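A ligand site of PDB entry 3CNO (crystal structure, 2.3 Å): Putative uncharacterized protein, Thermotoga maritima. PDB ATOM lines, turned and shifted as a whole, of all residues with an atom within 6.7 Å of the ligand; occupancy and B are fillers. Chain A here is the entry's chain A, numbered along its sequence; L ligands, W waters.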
ATOM      1  N   VAL A  28       7.974  12.847 -20.906  1.00  0.00           N
ATOM      2  CA  VAL A  28       8.027  11.568 -21.601  1.00  0.00           C
ATOM      3  C   VAL A  28       9.281  11.455 -22.435  1.00  0.00           C
ATOM      4  O   VAL A  28       9.387  12.045 -23.524  1.00  0.00           O
ATOM      5  CB  VAL A  28       6.767  11.313 -22.479  1.00  0.00           C
ATOM      6  CG1 VAL A  28       6.840   9.910 -23.106  1.00  0.00           C
ATOM      7  CG2 VAL A  28       5.486  11.486 -21.659  1.00  0.00           C
ATOM      8  N   ASN A  54      10.015   5.900 -21.164  1.00  0.00           N
ATOM      9  CA  ASN A  54       9.061   5.120 -21.969  1.00  0.00           C
ATOM     10  C   ASN A  54       9.748   4.152 -22.926  1.00  0.00           C
ATOM     11  O   ASN A  54      10.938   4.270 -23.188  1.00  0.00           O
ATOM     12  CB  ASN A  54       8.179   6.057 -22.803  1.00  0.00           C
ATOM     13  CG  ASN A  54       6.833   5.439 -23.156  1.00  0.00           C
ATOM     14  OD1 ASN A  54       6.358   4.529 -22.479  1.00  0.00           O
ATOM     15  ND2 ASN A  54       6.217   5.924 -24.222  1.00  0.00           N
ATOM     16  N   LYS A  55       8.959   3.217 -23.461  1.00  0.00           N
ATOM     17  CA  LYS A  55       9.432   2.237 -24.443  1.00  0.00           C
ATOM     18  C   LYS A  55      10.469   1.294 -23.859  1.00  0.00           C
ATOM     19  O   LYS A  55      11.412   0.893 -24.546  1.00  0.00           O
ATOM     20  CB  LYS A  55       9.953   2.923 -25.729  1.00  0.00           C
ATOM     21  CG  LYS A  55       9.006   3.955 -26.309  1.00  0.00           C
ATOM     22  CD  LYS A  55       9.423   4.397 -27.699  1.00  0.00           C
ATOM     23  CE  LYS A  55       8.379   5.342 -28.290  1.00  0.00           C
ATOM     24  NZ  LYS A  55       8.798   5.779 -29.630  1.00  0.00           N
ATOM     25  N   VAL A  56      10.282   0.933 -22.597  1.00  0.00           N
ATOM     26  CA  VAL A  56      11.216   0.012 -21.921  1.00  0.00           C
ATOM     27  C   VAL A  56      11.224  -1.371 -22.581  1.00  0.00           C
ATOM     28  O   VAL A  56      12.197  -2.101 -22.455  1.00  0.00           O
ATOM     29  CB  VAL A  56      10.989  -0.106 -20.382  1.00  0.00           C
ATOM     30  CG1 VAL A  56      11.426   1.164 -19.685  1.00  0.00           C
ATOM     31  CG2 VAL A  56       9.565  -0.436 -20.027  1.00  0.00           C
ATOM     32  N   ASP A  57      10.156  -1.688 -23.305  1.00  0.00           N
ATOM     33  CA  ASP A  57      10.028  -2.946 -24.055  1.00  0.00           C
ATOM     34  C   ASP A  57      11.026  -3.104 -25.196  1.00  0.00           C
ATOM     35  O   ASP A  57      11.334  -4.221 -25.615  1.00  0.00           O
ATOM     36  CB  ASP A  57       8.602  -3.060 -24.636  1.00  0.00           C
ATOM     37  CG  ASP A  57       8.234  -1.884 -25.561  1.00  0.00           C
ATOM     38  OD1 ASP A  57       8.358  -0.719 -25.127  1.00  0.00           O
ATOM     39  OD2 ASP A  57       7.797  -2.128 -26.707  1.00  0.00           O
ATOM     40  N   ILE A  58      11.528  -1.982 -25.727  1.00  0.00           N
ATOM     41  CA  ILE A  58      12.470  -2.044 -26.847  1.00  0.00           C
ATOM     42  C   ILE A  58      13.860  -1.501 -26.486  1.00  0.00           C
ATOM     43  O   ILE A  58      14.721  -1.317 -27.361  1.00  0.00           O
ATOM     44  CB  ILE A  58      11.901  -1.392 -28.144  1.00  0.00           C
ATOM     45  CG1 ILE A  58      11.527   0.076 -27.900  1.00  0.00           C
ATOM     46  CG2 ILE A  58      10.726  -2.210 -28.683  1.00  0.00           C
ATOM     47  CD1 ILE A  58      11.347   0.891 -29.180  1.00  0.00           C
ATOM     48  N   THR A  81       7.882   2.726 -18.101  1.00  0.00           N
ATOM     49  CA  THR A  81       6.652   2.170 -18.613  1.00  0.00           C
ATOM     50  C   THR A  81       6.756   1.882 -20.100  1.00  0.00           C
ATOM     51  O   THR A  81       7.776   2.173 -20.716  1.00  0.00           O
ATOM     52  CB  THR A  81       5.437   3.093 -18.281  1.00  0.00           C
ATOM     53  OG1 THR A  81       4.222   2.383 -18.557  1.00  0.00           O
ATOM     54  CG2 THR A  81       5.481   4.378 -19.091  1.00  0.00           C
ATOM     55  N   HIS A  82       5.717   1.309 -20.668  1.00  0.00           N
ATOM     56  CA  HIS A  82       5.658   1.062 -22.103  1.00  0.00           C
ATOM     57  C   HIS A  82       4.206   0.914 -22.538  1.00  0.00           C
ATOM     58  O   HIS A  82       3.310   0.835 -21.697  1.00  0.00           O
ATOM     59  CB  HIS A  82       6.496  -0.158 -22.512  1.00  0.00           C
ATOM     60  CG  HIS A  82       6.017  -1.447 -21.915  1.00  0.00           C
ATOM     61  ND1 HIS A  82       5.240  -2.354 -22.611  1.00  0.00           N
ATOM     62  CD2 HIS A  82       6.218  -1.984 -20.693  1.00  0.00           C
ATOM     63  CE1 HIS A  82       4.966  -3.388 -21.831  1.00  0.00           C
ATOM     64  NE2 HIS A  82       5.552  -3.185 -20.661  1.00  0.00           N
ATOM     65  N   LYS A  83       4.002   0.887 -23.855  1.00  0.00           N
ATOM     66  CA  LYS A  83       2.691   0.827 -24.487  1.00  0.00           C
ATOM     67  C   LYS A  83       1.795  -0.196 -23.813  1.00  0.00           C
ATOM     68  O   LYS A  83       0.671   0.117 -23.429  1.00  0.00           O
ATOM     69  CB  LYS A  83       2.870   0.446 -25.958  1.00  0.00           C
ATOM     70  CG  LYS A  83       2.024   1.237 -26.945  1.00  0.00           C
ATOM     71  CD  LYS A  83       2.113   0.648 -28.361  1.00  0.00           C
ATOM     72  CE  LYS A  83       3.492   0.061 -28.651  1.00  0.00           C
ATOM     73  NZ  LYS A  83       3.586  -0.714 -29.925  1.00  0.00           N
ATOM     74  N   GLY A  84       2.331  -1.402 -23.636  1.00  0.00           N
ATOM     75  CA  GLY A  84       1.573  -2.572 -23.212  1.00  0.00           C
ATOM     76  C   GLY A  84       1.328  -2.714 -21.718  1.00  0.00           C
ATOM     77  O   GLY A  84       0.678  -3.654 -21.291  1.00  0.00           O
ATOM     78  N   GLY A 106       7.316  16.418 -24.120  1.00  0.00           N
ATOM     79  CA  GLY A 106       8.453  15.708 -24.697  1.00  0.00           C
ATOM     80  C   GLY A 106       8.746  16.062 -26.143  1.00  0.00           C
ATOM     81  O   GLY A 106       8.015  16.821 -26.781  1.00  0.00           O
ATOM     82  N   VAL A 107       9.840  15.505 -26.654  1.00  0.00           N
ATOM     83  CA  VAL A 107      10.181  15.585 -28.085  1.00  0.00           C
ATOM     84  C   VAL A 107       9.226  14.715 -28.929  1.00  0.00           C
ATOM     85  O   VAL A 107       8.558  13.815 -28.395  1.00  0.00           O
ATOM     86  CB  VAL A 107      11.694  15.250 -28.333  1.00  0.00           C
ATOM     87  CG1 VAL A 107      12.588  16.159 -27.507  1.00  0.00           C
ATOM     88  CG2 VAL A 107      12.027  13.761 -28.055  1.00  0.00           C
ATOM     89  N   PRO A 108       9.129  14.991 -30.260  1.00  0.00           N
ATOM     90  CA  PRO A 108       8.264  14.150 -31.117  1.00  0.00           C
ATOM     91  C   PRO A 108       8.538  12.637 -31.037  1.00  0.00           C
ATOM     92  O   PRO A 108       9.684  12.230 -30.855  1.00  0.00           O
ATOM     93  CB  PRO A 108       8.577  14.663 -32.533  1.00  0.00           C
ATOM     94  CG  PRO A 108       8.982  16.097 -32.335  1.00  0.00           C
ATOM     95  CD  PRO A 108       9.756  16.084 -31.024  1.00  0.00           C
ATOM     96  N   ASN A 109       7.456  11.860 -31.162  1.00  0.00           N
ATOM     97  CA  ASN A 109       7.447  10.400 -31.351  1.00  0.00           C
ATOM     98  C   ASN A 109       7.931   9.519 -30.184  1.00  0.00           C
ATOM     99  O   ASN A 109       8.307   8.367 -30.337  1.00  0.00           O
ATOM    100  CB  ASN A 109       7.994  10.015 -32.729  1.00  0.00           C
ATOM    101  CG  ASN A 109       7.199  10.688 -33.858  1.00  0.00           C
ATOM    102  OD1 ASN A 109       5.961  10.583 -33.926  1.00  0.00           O
ATOM    103  ND2 ASN A 109       7.910  11.421 -34.729  1.00  0.00           N
ATOM    104  N   THR A 110       7.810  10.090 -28.999  1.00  0.00           N
ATOM    105  CA  THR A 110       8.384   9.537 -27.811  1.00  0.00           C
ATOM    106  C   THR A 110       7.312   8.730 -27.022  1.00  0.00           C
ATOM    107  O   THR A 110       7.618   8.005 -26.062  1.00  0.00           O
ATOM    108  CB  THR A 110       9.043  10.722 -27.057  1.00  0.00           C
ATOM    109  OG1 THR A 110      10.364  10.374 -26.603  1.00  0.00           O
ATOM    110  CG2 THR A 110       8.162  11.288 -25.975  1.00  0.00           C
ATOM    111  N   GLY A 111       6.064   8.839 -27.472  1.00  0.00           N
ATOM    112  CA  GLY A 111       4.975   7.966 -27.020  1.00  0.00           C
ATOM    113  C   GLY A 111       3.898   8.708 -26.231  1.00  0.00           C
ATOM    114  O   GLY A 111       3.119   8.095 -25.495  1.00  0.00           O
ATOM    115  N   LYS A 112       3.865  10.027 -26.421  1.00  0.00           N
ATOM    116  CA  LYS A 112       2.992  10.913 -25.666  1.00  0.00           C
ATOM    117  C   LYS A 112       1.506  10.748 -25.998  1.00  0.00           C
ATOM    118  O   LYS A 112       0.684  10.716 -25.071  1.00  0.00           O
ATOM    119  CB  LYS A 112       3.418  12.377 -25.849  1.00  0.00           C
ATOM    120  CG  LYS A 112       4.870  12.651 -25.444  1.00  0.00           C
ATOM    121  CD  LYS A 112       5.201  14.152 -25.483  1.00  0.00           C
ATOM    122  CE  LYS A 112       4.987  14.756 -26.888  1.00  0.00           C
ATOM    123  NZ  LYS A 112       5.877  14.131 -27.915  1.00  0.00           N
ATOM    124  N   SER A 113       1.149  10.655 -27.273  1.00  0.00           N
ATOM    125  CA  SER A 113      -0.253  10.438 -27.649  1.00  0.00           C
ATOM    126  C   SER A 113      -0.734   9.102 -27.104  1.00  0.00           C
ATOM    127  O   SER A 113      -1.805   9.024 -26.504  1.00  0.00           O
ATOM    128  CB  SER A 113      -0.442  10.441 -29.170  1.00  0.00           C
ATOM    129  OG  SER A 113       0.028  11.656 -29.728  1.00  0.00           O
ATOM    130  N   THR A 114       0.071   8.055 -27.317  1.00  0.00           N
ATOM    131  CA  THR A 114      -0.259   6.722 -26.816  1.00  0.00           C
ATOM    132  C   THR A 114      -0.551   6.758 -25.312  1.00  0.00           C
ATOM    133  O   THR A 114      -1.526   6.165 -24.861  1.00  0.00           O
ATOM    134  CB  THR A 114       0.861   5.729 -27.115  1.00  0.00           C
ATOM    135  OG1 THR A 114       1.211   5.855 -28.488  1.00  0.00           O
ATOM    136  CG2 THR A 114       0.423   4.316 -26.854  1.00  0.00           C
ATOM    137  N   ILE A 115       0.268   7.484 -24.556  1.00  0.00           N
ATOM    138  CA  ILE A 115       0.069   7.655 -23.117  1.00  0.00           C
ATOM    139  C   ILE A 115      -1.235   8.417 -22.799  1.00  0.00           C
ATOM    140  O   ILE A 115      -2.070   7.900 -22.028  1.00  0.00           O
ATOM    141  CB  ILE A 115       1.319   8.300 -22.436  1.00  0.00           C
ATOM    142  CG1 ILE A 115       2.455   7.269 -22.373  1.00  0.00           C
ATOM    143  CG2 ILE A 115       0.995   8.860 -21.033  1.00  0.00           C
ATOM    144  CD1 ILE A 115       3.792   7.858 -22.008  1.00  0.00           C
ATOM    145  N   ASN A 117      -3.852   8.676 -24.652  1.00  0.00           N
ATOM    146  CA  ASN A 117      -4.988   7.804 -25.013  1.00  0.00           C
ATOM    147  C   ASN A 117      -5.323   6.749 -23.962  1.00  0.00           C
ATOM    148  O   ASN A 117      -6.490   6.471 -23.726  1.00  0.00           O
ATOM    149  CB  ASN A 117      -4.771   7.135 -26.373  1.00  0.00           C
ATOM    150  CG  ASN A 117      -4.730   8.141 -27.514  1.00  0.00           C
ATOM    151  OD1 ASN A 117      -5.210   9.281 -27.384  1.00  0.00           O
ATOM    152  ND2 ASN A 117      -4.158   7.724 -28.642  1.00  0.00           N
ATOM    153  N   PRO A 152      -0.487  16.875 -25.791  1.00  0.00           N
ATOM    154  CA  PRO A 152       0.849  16.992 -25.189  1.00  0.00           C
ATOM    155  C   PRO A 152       1.600  18.183 -25.748  1.00  0.00           C
ATOM    156  O   PRO A 152       1.444  18.497 -26.926  1.00  0.00           O
ATOM    157  CB  PRO A 152       1.570  15.713 -25.639  1.00  0.00           C
ATOM    158  CG  PRO A 152       0.568  14.903 -26.413  1.00  0.00           C
ATOM    159  CD  PRO A 152      -0.556  15.794 -26.793  1.00  0.00           C
ATOM    160  N   ILE A 154       4.694  19.602 -27.386  1.00  0.00           N
ATOM    161  CA  ILE A 154       5.762  19.053 -28.232  1.00  0.00           C
ATOM    162  C   ILE A 154       6.996  19.952 -28.224  1.00  0.00           C
ATOM    163  O   ILE A 154       6.919  21.152 -28.479  1.00  0.00           O
ATOM    164  CB  ILE A 154       5.280  18.809 -29.687  1.00  0.00           C
ATOM    165  CG1 ILE A 154       3.922  18.078 -29.677  1.00  0.00           C
ATOM    166  CG2 ILE A 154       6.335  18.042 -30.479  1.00  0.00           C
ATOM    167  CD1 ILE A 154       3.283  17.932 -31.026  1.00  0.00           C
ATOM    168  N   ALA A 236      14.538   2.775 -34.640  1.00  0.00           N
ATOM    169  CA  ALA A 236      13.582   3.600 -33.874  1.00  0.00           C
ATOM    170  C   ALA A 236      12.296   2.863 -33.432  1.00  0.00           C
ATOM    171  O   ALA A 236      11.719   3.163 -32.387  1.00  0.00           O
ATOM    172  CB  ALA A 236      13.221   4.829 -34.682  1.00  0.00           C
ATOM    173  N   GLN A 237      11.857   1.902 -34.238  1.00  0.00           N
ATOM    174  CA  GLN A 237      10.689   1.080 -33.932  1.00  0.00           C
ATOM    175  C   GLN A 237      11.039  -0.120 -33.052  1.00  0.00           C
ATOM    176  O   GLN A 237      10.156  -0.871 -32.643  1.00  0.00           O
ATOM    177  CB  GLN A 237      10.037   0.581 -35.226  1.00  0.00           C
ATOM    178  CG  GLN A 237       9.522   1.682 -36.131  1.00  0.00           C
ATOM    179  CD  GLN A 237       8.817   1.120 -37.346  1.00  0.00           C
ATOM    180  OE1 GLN A 237       9.314   0.206 -37.997  1.00  0.00           O
ATOM    181  NE2 GLN A 237       7.665   1.684 -37.678  1.00  0.00           N
ATOM    182  N   GLY A 238      12.322  -0.301 -32.758  1.00  0.00           N
ATOM    183  CA  GLY A 238      12.770  -1.421 -31.923  1.00  0.00           C
ATOM    184  C   GLY A 238      12.800  -2.765 -32.644  1.00  0.00           C
ATOM    185  O   GLY A 238      12.848  -3.816 -32.002  1.00  0.00           O
HETATM  186  P1  LIG L   1       4.177  11.163 -29.814  1.00  0.00           P
HETATM  187  O1  LIG L   1       2.766  11.503 -29.423  1.00  0.00           O
HETATM  188  O2  LIG L   1       5.064  11.522 -28.634  1.00  0.00           O
HETATM  189  O3  LIG L   1       4.692  11.989 -30.974  1.00  0.00           O
HETATM  190  O4  LIG L   1       4.340   9.602 -30.135  1.00  0.00           O
HETATM  191  P2  LIG L   1       3.223   8.479 -30.384  1.00  0.00           P
HETATM  192  O5  LIG L   1       2.364   8.171 -29.188  1.00  0.00           O
HETATM  193  O6  LIG L   1       2.426   8.774 -31.621  1.00  0.00           O
HETATM  194  O7  LIG L   1       4.175   7.207 -30.637  1.00  0.00           O
HETATM  195  C1  LIG L   1       5.191   7.284 -31.632  1.00  0.00           C
HETATM  196  C2  LIG L   1       5.545   5.876 -32.080  1.00  0.00           C
HETATM  197  O8  LIG L   1       6.063   5.125 -30.984  1.00  0.00           O
HETATM  198  C3  LIG L   1       4.335   5.127 -32.584  1.00  0.00           C
HETATM  199  O9  LIG L   1       4.772   4.330 -33.697  1.00  0.00           O
HETATM  200  C4  LIG L   1       3.941   4.227 -31.439  1.00  0.00           C
HETATM  201  O10 LIG L   1       3.252   3.076 -31.946  1.00  0.00           O
HETATM  202  C5  LIG L   1       5.295   3.941 -30.782  1.00  0.00           C
HETATM  203  N1  LIG L   1       5.282   3.758 -29.306  1.00  0.00           N
HETATM  204  C6  LIG L   1       4.736   4.565 -28.380  1.00  0.00           C
HETATM  205  N2  LIG L   1       4.958   4.083 -27.132  1.00  0.00           N
HETATM  206  C7  LIG L   1       5.673   2.941 -27.257  1.00  0.00           C
HETATM  207  C8  LIG L   1       6.239   1.919 -26.345  1.00  0.00           C
HETATM  208  O11 LIG L   1       6.099   2.014 -25.110  1.00  0.00           O
HETATM  209  N3  LIG L   1       6.919   0.895 -26.887  1.00  0.00           N
HETATM  210  C9  LIG L   1       7.069   0.762 -28.222  1.00  0.00           C
HETATM  211  N4  LIG L   1       7.763  -0.301 -28.693  1.00  0.00           N
HETATM  212  N5  LIG L   1       6.574   1.649 -29.112  1.00  0.00           N
HETATM  213  C10 LIG L   1       5.883   2.735 -28.690  1.00  0.00           C
HETATM  214  O   HOH W   1       5.056  14.615 -30.715  1.00  0.00           O
HETATM  215  O   HOH W   2       7.809   1.604 -31.429  1.00  0.00           O
HETATM  216  O   HOH W   3      -0.528   8.703 -32.038  1.00  0.00           O
HETATM  217  O   HOH W   4       0.876   6.693 -33.081  1.00  0.00           O
HETATM  218  O   HOH W   5       3.381   5.144 -24.943  1.00  0.00           O
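Water W1 lies within hydrogen-bond range of an oxygen (O3) of the ligand (2.7 Å) and the side-chain amino group (NZ) of Lys 112 (3.0 Å).
Water W5 lies within hydrogen-bond range of a nitrogen (N2) of the ligand, the backbone carbonyl oxygen (O) of Gly 111 and the side-chain amide nitrogen (ND2) of Asn 54.
An oxygen (O1) of the ligand sits at hydrogen-bond distance from the side-chain hydroxyl (OG) of Ser 113.
An oxygen (O5) of the ligand is in hydrogen-bond range of the backbone NH (N) of Thr 114 (3.0 Å).
N of Thr 110 is in hydrogen-bond range of O2 of the ligand (3.1 Å).
The backbone NH (N) of Ser 113 is in hydrogen-bond range of an oxygen (O1) of the ligand, 2.8 Å away.
N of Lys 112 sits at hydrogen-bond distance from O2 of the ligand (2.9 Å).
The side-chain hydroxyl (OG1) of Thr 114 lies within hydrogen-bond range of an oxygen (O5) of the ligand (2.7 Å).
The backbone NH of Asn 109 lies within hydrogen-bond range of an oxygen (O3) of the ligand, at 2.8 Å.
The side-chain amino group of Lys 112 is in salt-bridge range of an oxygen (O2) of the ligand, 2.8 Å away.
An oxygen (O2) of the ligand lies within hydrogen-bond range of the backbone NH (N) of Gly 111, 3.1 Å away.
OD2 of Asp 57 lies within hydrogen-bond range of N4 of the ligand.
The backbone NH (N) of Lys 83 is in hydrogen-bond range of an oxygen (O11) of the ligand.
NZ of Lys 55 lies within hydrogen-bond range of O8 of the ligand (3.1 Å).
OD1 of Asn 54 touches O11 of the ligand, at 3.6 Å.
CG2 of Ile 58 touches N4 of the ligand (3.5 Å).
His 82 touches the ligand.
C of Pro 108 touches O3 of the ligand, at 3.9 Å.
Hydrophobic or aromatic side chains within 4 Å of the ligand: Ile 58 and His 82.
Within 4 Å of the ligand: Asn 54, Lys 55, Asp 57, Ile 58, His 82, Lys 83, Pro 108, Asn 109, Thr 110, Gly 111, Lys 112, Ser 113 and Thr 114.
The nearest printed residue that does not touch the ligand is Val 107 (4.2 Å).
The backbone carbonyl oxygen (O) of Thr 110 is in hydrogen-bond range of the side-chain amide nitrogen (ND2) of Asn 54 (3.1 Å).
The side-chain amide oxygen (OD1) of Asn 54 sits close to the backbone carbonyl oxygen (O) of Thr 81 (3.3 Å).
NZ of Lys 112 is in hydrogen-bond range of O of Val 107 (2.7 Å).
The backbone carbonyl oxygen of Ser 113 sits close to the side-chain amide nitrogen of Asn 117.
A ring nitrogen (ND1) of His 82 sits close to the backbone NH (N) of Gly 84, at 3.2 Å.
NZ of Lys 55 lies within hydrogen-bond range of O of Asn 109.
N of Lys 55 sits at hydrogen-bond distance from O of Thr 81 (3.2 Å).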
